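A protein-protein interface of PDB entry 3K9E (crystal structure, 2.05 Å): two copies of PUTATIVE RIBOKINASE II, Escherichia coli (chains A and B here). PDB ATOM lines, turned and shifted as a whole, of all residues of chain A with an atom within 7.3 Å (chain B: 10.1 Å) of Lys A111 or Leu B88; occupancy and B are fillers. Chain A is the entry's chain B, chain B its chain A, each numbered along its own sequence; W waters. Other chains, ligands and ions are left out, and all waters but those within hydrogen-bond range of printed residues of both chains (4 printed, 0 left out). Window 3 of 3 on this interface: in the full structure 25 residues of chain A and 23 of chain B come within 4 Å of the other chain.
NZ of Lys A111 sits at hydrogen-bond distance from O of Leu B88 (2.9 Å).
The side-chain amide nitrogen of Asn A109 sits close to the side-chain amide nitrogen of Asn B109 (3.4 Å).
N of Ala B114 lies within hydrogen-bond range of O of Ala B90 (2.8 Å).
Among the printed residues, pairs that only touch across the chains: Glu A89 with Asn B112, Phe A108 with Ala B90, Asn A112 with Leu B88, Asn A112 with Glu B89 and Asn A112 with Asn B112.
No residue of chain B comes within 4 Å of Ile A110.
Of chain B, only Leu B88 (2.9 Å) comes within 4 Å of Lys A111.
Of chain B, only Leu B88, Glu B89 and Asn B112 come within 4 Å of Asn A112.
Gly A116 touches none of the printed residues of chain B.
Leu B88 touches just these residues of chain A: Lys A111 (2.9 Å) and Asn A112 (3.6 Å).
Printed residues of chain A within 4 Å of Glu B89: Asn A112.
Printed residues of chain A within 4 Å of Ala B90: Phe A108 (3.8 Å).
The nearest residue of chain B that does not touch Lys A111 is Glu B89 (4.9 Å).
The nearest residue of chain A that does not touch Leu B88 is Phe A108 (7.1 Å).
The nearest printed residue of chain A that does not touch Asn B112 is Asn A109 (5.0 Å).
Of the 16 printed residues of chain A, 5 touch a printed residue of chain B.
Along chain A the printed residues that touch a printed residue of chain B span positions 89 to 112.
Glu A89 touches Asn B112, and with the chains exchanged Asn A112 touches Glu B89.
Asn A109 touches its own counterpart, Asn B109.
Asn B112 touches its own counterpart, Asn A112.
7 positions are printed for both chains.
Of the 7 pairs that touch across the chains among the printed residues, 4 have their exchanged pair printed and touching as well.
Water W1 lies within hydrogen-bond range of the side-chain amide oxygen (OD1) of Asn A109 (2.6 Å), the backbone carbonyl oxygen (O) of Asn B112 (2.8 Å) and the side-chain amide nitrogen (ND2) of Asn B109 (3.1 Å).
Water W2 lies within hydrogen-bond range of OD1 of Asn B109 (2.7 Å), O of Asn A112 (2.7 Å) and ND2 of Asn A109 (3.3 Å).
Water W3 bridges the side-chain amide oxygen (OD1) of Asn B112 and the side-chain carboxylate (OE1) of Glu A89.
Water W4 lies within hydrogen-bond range of ND2 of Asn A112 (2.8 Å), OE1 of Glu B89 (3.0 Å) and N of Ala B90 (3.1 Å).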
ATOM      1  N   GLU A  89      11.297  -6.395   3.298  1.00  0.00           N
ATOM      2  CA  GLU A  89      10.985  -6.887   4.636  1.00  0.00           C
ATOM      3  C   GLU A  89      11.008  -8.412   4.690  1.00  0.00           C
ATOM      4  O   GLU A  89      10.832  -9.081   3.673  1.00  0.00           O
ATOM      5  CB  GLU A  89       9.603  -6.385   5.071  1.00  0.00           C
ATOM      6  CG  GLU A  89       9.487  -4.877   5.221  1.00  0.00           C
ATOM      7  CD  GLU A  89      10.337  -4.335   6.357  1.00  0.00           C
ATOM      8  OE1 GLU A  89      10.182  -4.815   7.506  1.00  0.00           O
ATOM      9  OE2 GLU A  89      11.156  -3.422   6.110  1.00  0.00           O
ATOM     10  N   GLY A  92       7.345 -12.297   8.987  1.00  0.00           N
ATOM     11  CA  GLY A  92       7.423 -12.558  10.411  1.00  0.00           C
ATOM     12  C   GLY A  92       7.559 -14.037  10.719  1.00  0.00           C
ATOM     13  O   GLY A  92       7.158 -14.890   9.917  1.00  0.00           O
ATOM     14  N   PHE A 108      10.059 -14.257  19.124  1.00  0.00           N
ATOM     15  CA  PHE A 108       9.228 -13.615  18.118  1.00  0.00           C
ATOM     16  C   PHE A 108       9.920 -12.584  17.255  1.00  0.00           C
ATOM     17  O   PHE A 108      10.809 -11.868  17.706  1.00  0.00           O
ATOM     18  CB  PHE A 108       8.053 -12.885  18.776  1.00  0.00           C
ATOM     19  CG  PHE A 108       7.003 -13.784  19.343  1.00  0.00           C
ATOM     20  CD1 PHE A 108       6.286 -14.638  18.523  1.00  0.00           C
ATOM     21  CD2 PHE A 108       6.692 -13.732  20.695  1.00  0.00           C
ATOM     22  CE1 PHE A 108       5.268 -15.427  19.040  1.00  0.00           C
ATOM     23  CE2 PHE A 108       5.677 -14.517  21.221  1.00  0.00           C
ATOM     24  CZ  PHE A 108       4.963 -15.365  20.394  1.00  0.00           C
ATOM     25  N   ASN A 109       9.483 -12.521  16.005  1.00  0.00           N
ATOM     26  CA  ASN A 109       9.938 -11.516  15.069  1.00  0.00           C
ATOM     27  C   ASN A 109       8.675 -11.178  14.307  1.00  0.00           C
ATOM     28  O   ASN A 109       8.348 -11.803  13.305  1.00  0.00           O
ATOM     29  CB  ASN A 109      11.005 -12.012  14.101  1.00  0.00           C
ATOM     30  CG  ASN A 109      11.460 -10.896  13.161  1.00  0.00           C
ATOM     31  OD1 ASN A 109      11.620  -9.747  13.588  1.00  0.00           O
ATOM     32  ND2 ASN A 109      11.663 -11.221  11.893  1.00  0.00           N
ATOM     33  N   ILE A 110       7.950 -10.198  14.822  1.00  0.00           N
ATOM     34  CA  ILE A 110       6.699  -9.772  14.223  1.00  0.00           C
ATOM     35  C   ILE A 110       6.646  -8.248  14.135  1.00  0.00           C
ATOM     36  O   ILE A 110       6.346  -7.677  13.082  1.00  0.00           O
ATOM     37  CB  ILE A 110       5.525 -10.256  15.084  1.00  0.00           C
ATOM     38  CG1 ILE A 110       5.503 -11.786  15.104  1.00  0.00           C
ATOM     39  CG2 ILE A 110       4.224  -9.664  14.577  1.00  0.00           C
ATOM     40  CD1 ILE A 110       4.543 -12.363  16.108  1.00  0.00           C
ATOM     41  N   LYS A 111       6.949  -7.604  15.255  1.00  0.00           N
ATOM     42  CA  LYS A 111       6.913  -6.152  15.355  1.00  0.00           C
ATOM     43  C   LYS A 111       7.866  -5.442  14.392  1.00  0.00           C
ATOM     44  O   LYS A 111       7.521  -4.398  13.833  1.00  0.00           O
ATOM     45  CB  LYS A 111       7.221  -5.743  16.796  1.00  0.00           C
ATOM     46  CG  LYS A 111       7.230  -4.252  17.038  1.00  0.00           C
ATOM     47  CD  LYS A 111       8.530  -3.817  17.703  1.00  0.00           C
ATOM     48  CE  LYS A 111       8.823  -4.603  18.977  1.00  0.00           C
ATOM     49  NZ  LYS A 111      10.153  -4.235  19.559  1.00  0.00           N
ATOM     50  N   ASN A 112       9.060  -6.004  14.206  1.00  0.00           N
ATOM     51  CA  ASN A 112      10.053  -5.418  13.316  1.00  0.00           C
ATOM     52  C   ASN A 112      10.204  -6.213  12.036  1.00  0.00           C
ATOM     53  O   ASN A 112      11.267  -6.208  11.414  1.00  0.00           O
ATOM     54  CB  ASN A 112      11.417  -5.324  14.010  1.00  0.00           C
ATOM     55  CG  ASN A 112      11.354  -4.553  15.309  1.00  0.00           C
ATOM     56  OD1 ASN A 112      10.814  -3.458  15.356  1.00  0.00           O
ATOM     57  ND2 ASN A 112      11.902  -5.128  16.374  1.00  0.00           N
ATOM     58  N   ALA A 113       9.144  -6.909  11.649  1.00  0.00           N
ATOM     59  CA  ALA A 113       9.162  -7.698  10.425  1.00  0.00           C
ATOM     60  C   ALA A 113       8.042  -7.190   9.519  1.00  0.00           C
ATOM     61  O   ALA A 113       7.366  -6.211   9.846  1.00  0.00           O
ATOM     62  CB  ALA A 113       8.966  -9.175  10.751  1.00  0.00           C
ATOM     63  N   ALA A 114       7.843  -7.846   8.381  1.00  0.00           N
ATOM     64  CA  ALA A 114       6.799  -7.432   7.452  1.00  0.00           C
ATOM     65  C   ALA A 114       5.480  -7.097   8.153  1.00  0.00           C
ATOM     66  O   ALA A 114       4.867  -6.072   7.857  1.00  0.00           O
ATOM     67  CB  ALA A 114       6.579  -8.509   6.400  1.00  0.00           C
ATOM     68  N   CYS A 115       5.059  -7.946   9.091  1.00  0.00           N
ATOM     69  CA  CYS A 115       3.805  -7.740   9.821  1.00  0.00           C
ATOM     70  C   CYS A 115       3.656  -6.334  10.381  1.00  0.00           C
ATOM     71  O   CYS A 115       2.646  -5.672  10.152  1.00  0.00           O
ATOM     72  CB  CYS A 115       3.681  -8.703  11.005  1.00  0.00           C
ATOM     73  SG  CYS A 115       4.575 -10.228  10.873  1.00  0.00           S
ATOM     74  N   GLY A 116       4.657  -5.900  11.147  1.00  0.00           N
ATOM     75  CA  GLY A 116       4.622  -4.582  11.758  1.00  0.00           C
ATOM     76  C   GLY A 116       4.730  -3.440  10.768  1.00  0.00           C
ATOM     77  O   GLY A 116       4.835  -2.277  11.165  1.00  0.00           O
ATOM     78  N   LYS A 117       4.703  -3.772   9.479  1.00  0.00           N
ATOM     79  CA  LYS A 117       4.795  -2.774   8.416  1.00  0.00           C
ATOM     80  C   LYS A 117       3.399  -2.352   7.957  1.00  0.00           C
ATOM     81  O   LYS A 117       3.207  -1.252   7.442  1.00  0.00           O
ATOM     82  CB  LYS A 117       5.556  -3.351   7.223  1.00  0.00           C
ATOM     83  CG  LYS A 117       6.591  -2.424   6.609  1.00  0.00           C
ATOM     84  CD  LYS A 117       7.954  -2.577   7.276  1.00  0.00           C
ATOM     85  CE  LYS A 117       7.995  -1.983   8.673  1.00  0.00           C
ATOM     86  NZ  LYS A 117       7.949  -0.497   8.645  1.00  0.00           N
ATOM     87  N   PHE A 142      -0.094  -3.438  17.985  1.00  0.00           N
ATOM     88  CA  PHE A 142       1.162  -3.223  18.689  1.00  0.00           C
ATOM     89  C   PHE A 142       1.963  -2.052  18.127  1.00  0.00           C
ATOM     90  O   PHE A 142       3.167  -1.947  18.362  1.00  0.00           O
ATOM     91  CB  PHE A 142       2.003  -4.506  18.669  1.00  0.00           C
ATOM     92  CG  PHE A 142       2.176  -5.110  17.298  1.00  0.00           C
ATOM     93  CD1 PHE A 142       3.010  -4.519  16.358  1.00  0.00           C
ATOM     94  CD2 PHE A 142       1.516  -6.287  16.960  1.00  0.00           C
ATOM     95  CE1 PHE A 142       3.190  -5.095  15.098  1.00  0.00           C
ATOM     96  CE2 PHE A 142       1.688  -6.871  15.706  1.00  0.00           C
ATOM     97  CZ  PHE A 142       2.525  -6.276  14.774  1.00  0.00           C
ATOM     98  N   SER A 143       1.290  -1.175  17.386  1.00  0.00           N
ATOM     99  CA  SER A 143       1.932   0.003  16.808  1.00  0.00           C
ATOM    100  C   SER A 143       0.850   0.952  16.312  1.00  0.00           C
ATOM    101  O   SER A 143      -0.279   0.528  16.051  1.00  0.00           O
ATOM    102  CB  SER A 143       2.846  -0.385  15.645  1.00  0.00           C
ATOM    103  OG  SER A 143       2.132  -0.442  14.424  1.00  0.00           O
ATOM    104  N   MET A 146      -0.507   0.104  12.924  1.00  0.00           N
ATOM    105  CA  MET A 146      -1.473  -0.984  12.947  1.00  0.00           C
ATOM    106  C   MET A 146      -2.864  -0.446  13.258  1.00  0.00           C
ATOM    107  O   MET A 146      -3.824  -0.739  12.542  1.00  0.00           O
ATOM    108  CB  MET A 146      -1.097  -2.028  14.005  1.00  0.00           C
ATOM    109  CG  MET A 146       0.341  -2.543  13.944  1.00  0.00           C
ATOM    110  SD  MET A 146       0.896  -3.326  12.251  1.00  0.00           S
ATOM    111  CE  MET A 146       1.922  -1.825  11.569  1.00  0.00           C
ATOM    112  N   ARG A 171      -1.291  -8.883  24.440  1.00  0.00           N
ATOM    113  CA  ARG A 171      -0.244  -9.122  25.418  1.00  0.00           C
ATOM    114  C   ARG A 171      -0.552  -8.090  26.501  1.00  0.00           C
ATOM    115  O   ARG A 171      -0.721  -6.906  26.206  1.00  0.00           O
ATOM    116  CB  ARG A 171       1.130  -8.849  24.811  1.00  0.00           C
ATOM    117  CG  ARG A 171       1.602  -9.887  23.807  1.00  0.00           C
ATOM    118  CD  ARG A 171       2.873  -9.405  23.114  1.00  0.00           C
ATOM    119  NE  ARG A 171       3.909  -9.009  24.066  1.00  0.00           N
ATOM    120  CZ  ARG A 171       4.972  -8.271  23.753  1.00  0.00           C
ATOM    121  NH1 ARG A 171       5.146  -7.846  22.507  1.00  0.00           N
ATOM    122  NH2 ARG A 171       5.860  -7.952  24.690  1.00  0.00           N
ATOM    123  N   VAL B  60      23.013  -8.044  19.792  1.00  0.00           N
ATOM    124  CA  VAL B  60      22.151  -9.212  19.686  1.00  0.00           C
ATOM    125  C   VAL B  60      20.922  -8.934  20.534  1.00  0.00           C
ATOM    126  O   VAL B  60      20.871  -7.928  21.241  1.00  0.00           O
ATOM    127  CB  VAL B  60      22.838 -10.489  20.214  1.00  0.00           C
ATOM    128  CG1 VAL B  60      24.100 -10.785  19.397  1.00  0.00           C
ATOM    129  CG2 VAL B  60      23.172 -10.325  21.686  1.00  0.00           C
ATOM    130  N   GLY B  61      19.929  -9.815  20.460  1.00  0.00           N
ATOM    131  CA  GLY B  61      18.735  -9.622  21.261  1.00  0.00           C
ATOM    132  C   GLY B  61      18.878 -10.339  22.592  1.00  0.00           C
ATOM    133  O   GLY B  61      19.828 -11.092  22.809  1.00  0.00           O
ATOM    134  N   ASN B  62      17.938 -10.103  23.498  1.00  0.00           N
ATOM    135  CA  ASN B  62      17.974 -10.752  24.799  1.00  0.00           C
ATOM    136  C   ASN B  62      17.203 -12.059  24.657  1.00  0.00           C
ATOM    137  O   ASN B  62      16.116 -12.220  25.214  1.00  0.00           O
ATOM    138  CB  ASN B  62      17.337  -9.829  25.843  1.00  0.00           C
ATOM    139  CG  ASN B  62      17.134 -10.501  27.180  1.00  0.00           C
ATOM    140  OD1 ASN B  62      17.993 -11.230  27.665  1.00  0.00           O
ATOM    141  ND2 ASN B  62      15.989 -10.240  27.796  1.00  0.00           N
ATOM    142  N   ASP B  63      17.771 -12.974  23.872  1.00  0.00           N
ATOM    143  CA  ASP B  63      17.162 -14.276  23.617  1.00  0.00           C
ATOM    144  C   ASP B  63      18.216 -15.375  23.451  1.00  0.00           C
ATOM    145  O   ASP B  63      19.418 -15.106  23.409  1.00  0.00           O
ATOM    146  CB  ASP B  63      16.263 -14.211  22.369  1.00  0.00           C
ATOM    147  CG  ASP B  63      16.996 -13.689  21.137  1.00  0.00           C
ATOM    148  OD1 ASP B  63      18.150 -14.100  20.900  1.00  0.00           O
ATOM    149  OD2 ASP B  63      16.408 -12.879  20.388  1.00  0.00           O
ATOM    150  N   SER B  84      26.581  -5.746  22.765  1.00  0.00           N
ATOM    151  CA  SER B  84      25.450  -5.154  23.468  1.00  0.00           C
ATOM    152  C   SER B  84      24.201  -6.006  23.276  1.00  0.00           C
ATOM    153  O   SER B  84      23.975  -6.563  22.197  1.00  0.00           O
ATOM    154  CB  SER B  84      25.177  -3.745  22.947  1.00  0.00           C
ATOM    155  OG  SER B  84      26.179  -2.844  23.378  1.00  0.00           O
ATOM    156  N   VAL B  85      23.389  -6.109  24.323  1.00  0.00           N
ATOM    157  CA  VAL B  85      22.154  -6.880  24.244  1.00  0.00           C
ATOM    158  C   VAL B  85      20.972  -5.919  24.184  1.00  0.00           C
ATOM    159  O   VAL B  85      20.792  -5.085  25.074  1.00  0.00           O
ATOM    160  CB  VAL B  85      22.013  -7.825  25.451  1.00  0.00           C
ATOM    161  CG1 VAL B  85      20.653  -8.531  25.423  1.00  0.00           C
ATOM    162  CG2 VAL B  85      23.137  -8.847  25.424  1.00  0.00           C
ATOM    163  N   LEU B  86      20.181  -6.040  23.119  1.00  0.00           N
ATOM    164  CA  LEU B  86      19.026  -5.189  22.898  1.00  0.00           C
ATOM    165  C   LEU B  86      17.715  -5.916  23.203  1.00  0.00           C
ATOM    166  O   LEU B  86      17.282  -6.780  22.441  1.00  0.00           O
ATOM    167  CB  LEU B  86      19.033  -4.688  21.452  1.00  0.00           C
ATOM    168  CG  LEU B  86      20.011  -3.558  21.111  1.00  0.00           C
ATOM    169  CD1 LEU B  86      21.401  -3.877  21.626  1.00  0.00           C
ATOM    170  CD2 LEU B  86      20.043  -3.351  19.609  1.00  0.00           C
ATOM    171  N   PRO B  87      17.064  -5.558  24.327  1.00  0.00           N
ATOM    172  CA  PRO B  87      15.798  -6.127  24.814  1.00  0.00           C
ATOM    173  C   PRO B  87      14.632  -6.127  23.832  1.00  0.00           C
ATOM    174  O   PRO B  87      13.863  -7.085  23.774  1.00  0.00           O
ATOM    175  CB  PRO B  87      15.485  -5.277  26.046  1.00  0.00           C
ATOM    176  CG  PRO B  87      16.827  -4.865  26.530  1.00  0.00           C
ATOM    177  CD  PRO B  87      17.553  -4.521  25.253  1.00  0.00           C
ATOM    178  N   LEU B  88      14.502  -5.057  23.063  1.00  0.00           N
ATOM    179  CA  LEU B  88      13.399  -4.938  22.117  1.00  0.00           C
ATOM    180  C   LEU B  88      13.697  -5.475  20.717  1.00  0.00           C
ATOM    181  O   LEU B  88      12.848  -5.403  19.824  1.00  0.00           O
ATOM    182  CB  LEU B  88      12.985  -3.468  22.022  1.00  0.00           C
ATOM    183  CG  LEU B  88      12.785  -2.800  23.389  1.00  0.00           C
ATOM    184  CD1 LEU B  88      12.653  -1.284  23.240  1.00  0.00           C
ATOM    185  CD2 LEU B  88      11.555  -3.408  24.058  1.00  0.00           C
ATOM    186  N   GLU B  89      14.894  -6.020  20.523  1.00  0.00           N
ATOM    187  CA  GLU B  89      15.270  -6.541  19.215  1.00  0.00           C
ATOM    188  C   GLU B  89      15.520  -8.043  19.230  1.00  0.00           C
ATOM    189  O   GLU B  89      15.967  -8.596  20.229  1.00  0.00           O
ATOM    190  CB  GLU B  89      16.531  -5.838  18.717  1.00  0.00           C
ATOM    191  CG  GLU B  89      16.446  -4.324  18.678  1.00  0.00           C
ATOM    192  CD  GLU B  89      15.386  -3.820  17.727  1.00  0.00           C
ATOM    193  OE1 GLU B  89      15.322  -4.312  16.578  1.00  0.00           O
ATOM    194  OE2 GLU B  89      14.621  -2.920  18.122  1.00  0.00           O
ATOM    195  N   ALA B  90      15.223  -8.703  18.115  1.00  0.00           N
ATOM    196  CA  ALA B  90      15.458 -10.136  18.000  1.00  0.00           C
ATOM    197  C   ALA B  90      16.860 -10.302  17.417  1.00  0.00           C
ATOM    198  O   ALA B  90      17.284  -9.515  16.568  1.00  0.00           O
ATOM    199  CB  ALA B  90      14.427 -10.775  17.070  1.00  0.00           C
ATOM    200  N   THR B  91      17.592 -11.302  17.890  1.00  0.00           N
ATOM    201  CA  THR B  91      18.928 -11.550  17.369  1.00  0.00           C
ATOM    202  C   THR B  91      18.734 -11.905  15.896  1.00  0.00           C
ATOM    203  O   THR B  91      17.726 -12.511  15.526  1.00  0.00           O
ATOM    204  CB  THR B  91      19.588 -12.715  18.118  1.00  0.00           C
ATOM    205  OG1 THR B  91      19.681 -12.387  19.515  1.00  0.00           O
ATOM    206  CG2 THR B  91      20.980 -12.991  17.557  1.00  0.00           C
ATOM    207  N   ASN B 109      17.337 -12.289   8.169  1.00  0.00           N
ATOM    208  CA  ASN B 109      16.746 -11.306   9.068  1.00  0.00           C
ATOM    209  C   ASN B 109      17.950 -10.709   9.789  1.00  0.00           C
ATOM    210  O   ASN B 109      18.310 -11.149  10.877  1.00  0.00           O
ATOM    211  CB  ASN B 109      15.798 -11.888  10.112  1.00  0.00           C
ATOM    212  CG  ASN B 109      15.162 -10.778  10.955  1.00  0.00           C
ATOM    213  OD1 ASN B 109      14.803  -9.726  10.415  1.00  0.00           O
ATOM    214  ND2 ASN B 109      15.036 -10.993  12.258  1.00  0.00           N
ATOM    215  N   ASN B 112      16.815  -5.642   9.667  1.00  0.00           N
ATOM    216  CA  ASN B 112      15.764  -5.238  10.591  1.00  0.00           C
ATOM    217  C   ASN B 112      15.812  -5.997  11.910  1.00  0.00           C
ATOM    218  O   ASN B 112      14.832  -6.026  12.646  1.00  0.00           O
ATOM    219  CB  ASN B 112      14.404  -5.429   9.904  1.00  0.00           C
ATOM    220  CG  ASN B 112      14.302  -4.647   8.601  1.00  0.00           C
ATOM    221  OD1 ASN B 112      13.939  -5.192   7.551  1.00  0.00           O
ATOM    222  ND2 ASN B 112      14.629  -3.362   8.664  1.00  0.00           N
ATOM    223  N   ALA B 113      16.962  -6.599  12.200  1.00  0.00           N
ATOM    224  CA  ALA B 113      17.164  -7.355  13.432  1.00  0.00           C
ATOM    225  C   ALA B 113      18.145  -6.610  14.344  1.00  0.00           C
ATOM    226  O   ALA B 113      18.693  -5.561  13.974  1.00  0.00           O
ATOM    227  CB  ALA B 113      17.708  -8.745  13.105  1.00  0.00           C
ATOM    228  N   ALA B 114      18.375  -7.170  15.526  1.00  0.00           N
ATOM    229  CA  ALA B 114      19.270  -6.567  16.507  1.00  0.00           C
ATOM    230  C   ALA B 114      20.596  -6.122  15.912  1.00  0.00           C
ATOM    231  O   ALA B 114      21.005  -4.974  16.102  1.00  0.00           O
ATOM    232  CB  ALA B 114      19.516  -7.534  17.669  1.00  0.00           C
ATOM    233  N   CYS B 115      21.270  -7.020  15.198  1.00  0.00           N
ATOM    234  CA  CYS B 115      22.555  -6.672  14.609  1.00  0.00           C
ATOM    235  C   CYS B 115      22.455  -5.472  13.676  1.00  0.00           C
ATOM    236  O   CYS B 115      23.459  -4.820  13.377  1.00  0.00           O
ATOM    237  CB  CYS B 115      23.171  -7.877  13.882  1.00  0.00           C
ATOM    238  SG  CYS B 115      22.054  -8.886  12.878  1.00  0.00           S
ATOM    239  N   LYS B 117      20.974  -2.745  14.445  1.00  0.00           N
ATOM    240  CA  LYS B 117      20.794  -1.543  15.264  1.00  0.00           C
ATOM    241  C   LYS B 117      22.118  -1.002  15.773  1.00  0.00           C
ATOM    242  O   LYS B 117      22.152  -0.002  16.497  1.00  0.00           O
ATOM    243  CB  LYS B 117      19.910  -1.857  16.470  1.00  0.00           C
ATOM    244  CG  LYS B 117      18.650  -2.608  16.126  1.00  0.00           C
ATOM    245  CD  LYS B 117      17.770  -1.792  15.217  1.00  0.00           C
ATOM    246  CE  LYS B 117      17.285  -0.520  15.883  1.00  0.00           C
ATOM    247  NZ  LYS B 117      16.131   0.044  15.116  1.00  0.00           N
HETATM  248  O   HOH W   1      13.851  -8.496  13.659  1.00  0.00           O
HETATM  249  O   HOH W   2      12.488  -8.387  10.432  1.00  0.00           O
HETATM  250  O   HOH W   3      12.124  -7.131   7.927  1.00  0.00           O
HETATM  251  O   HOH W   4      13.967  -6.921  15.949  1.00  0.00           O
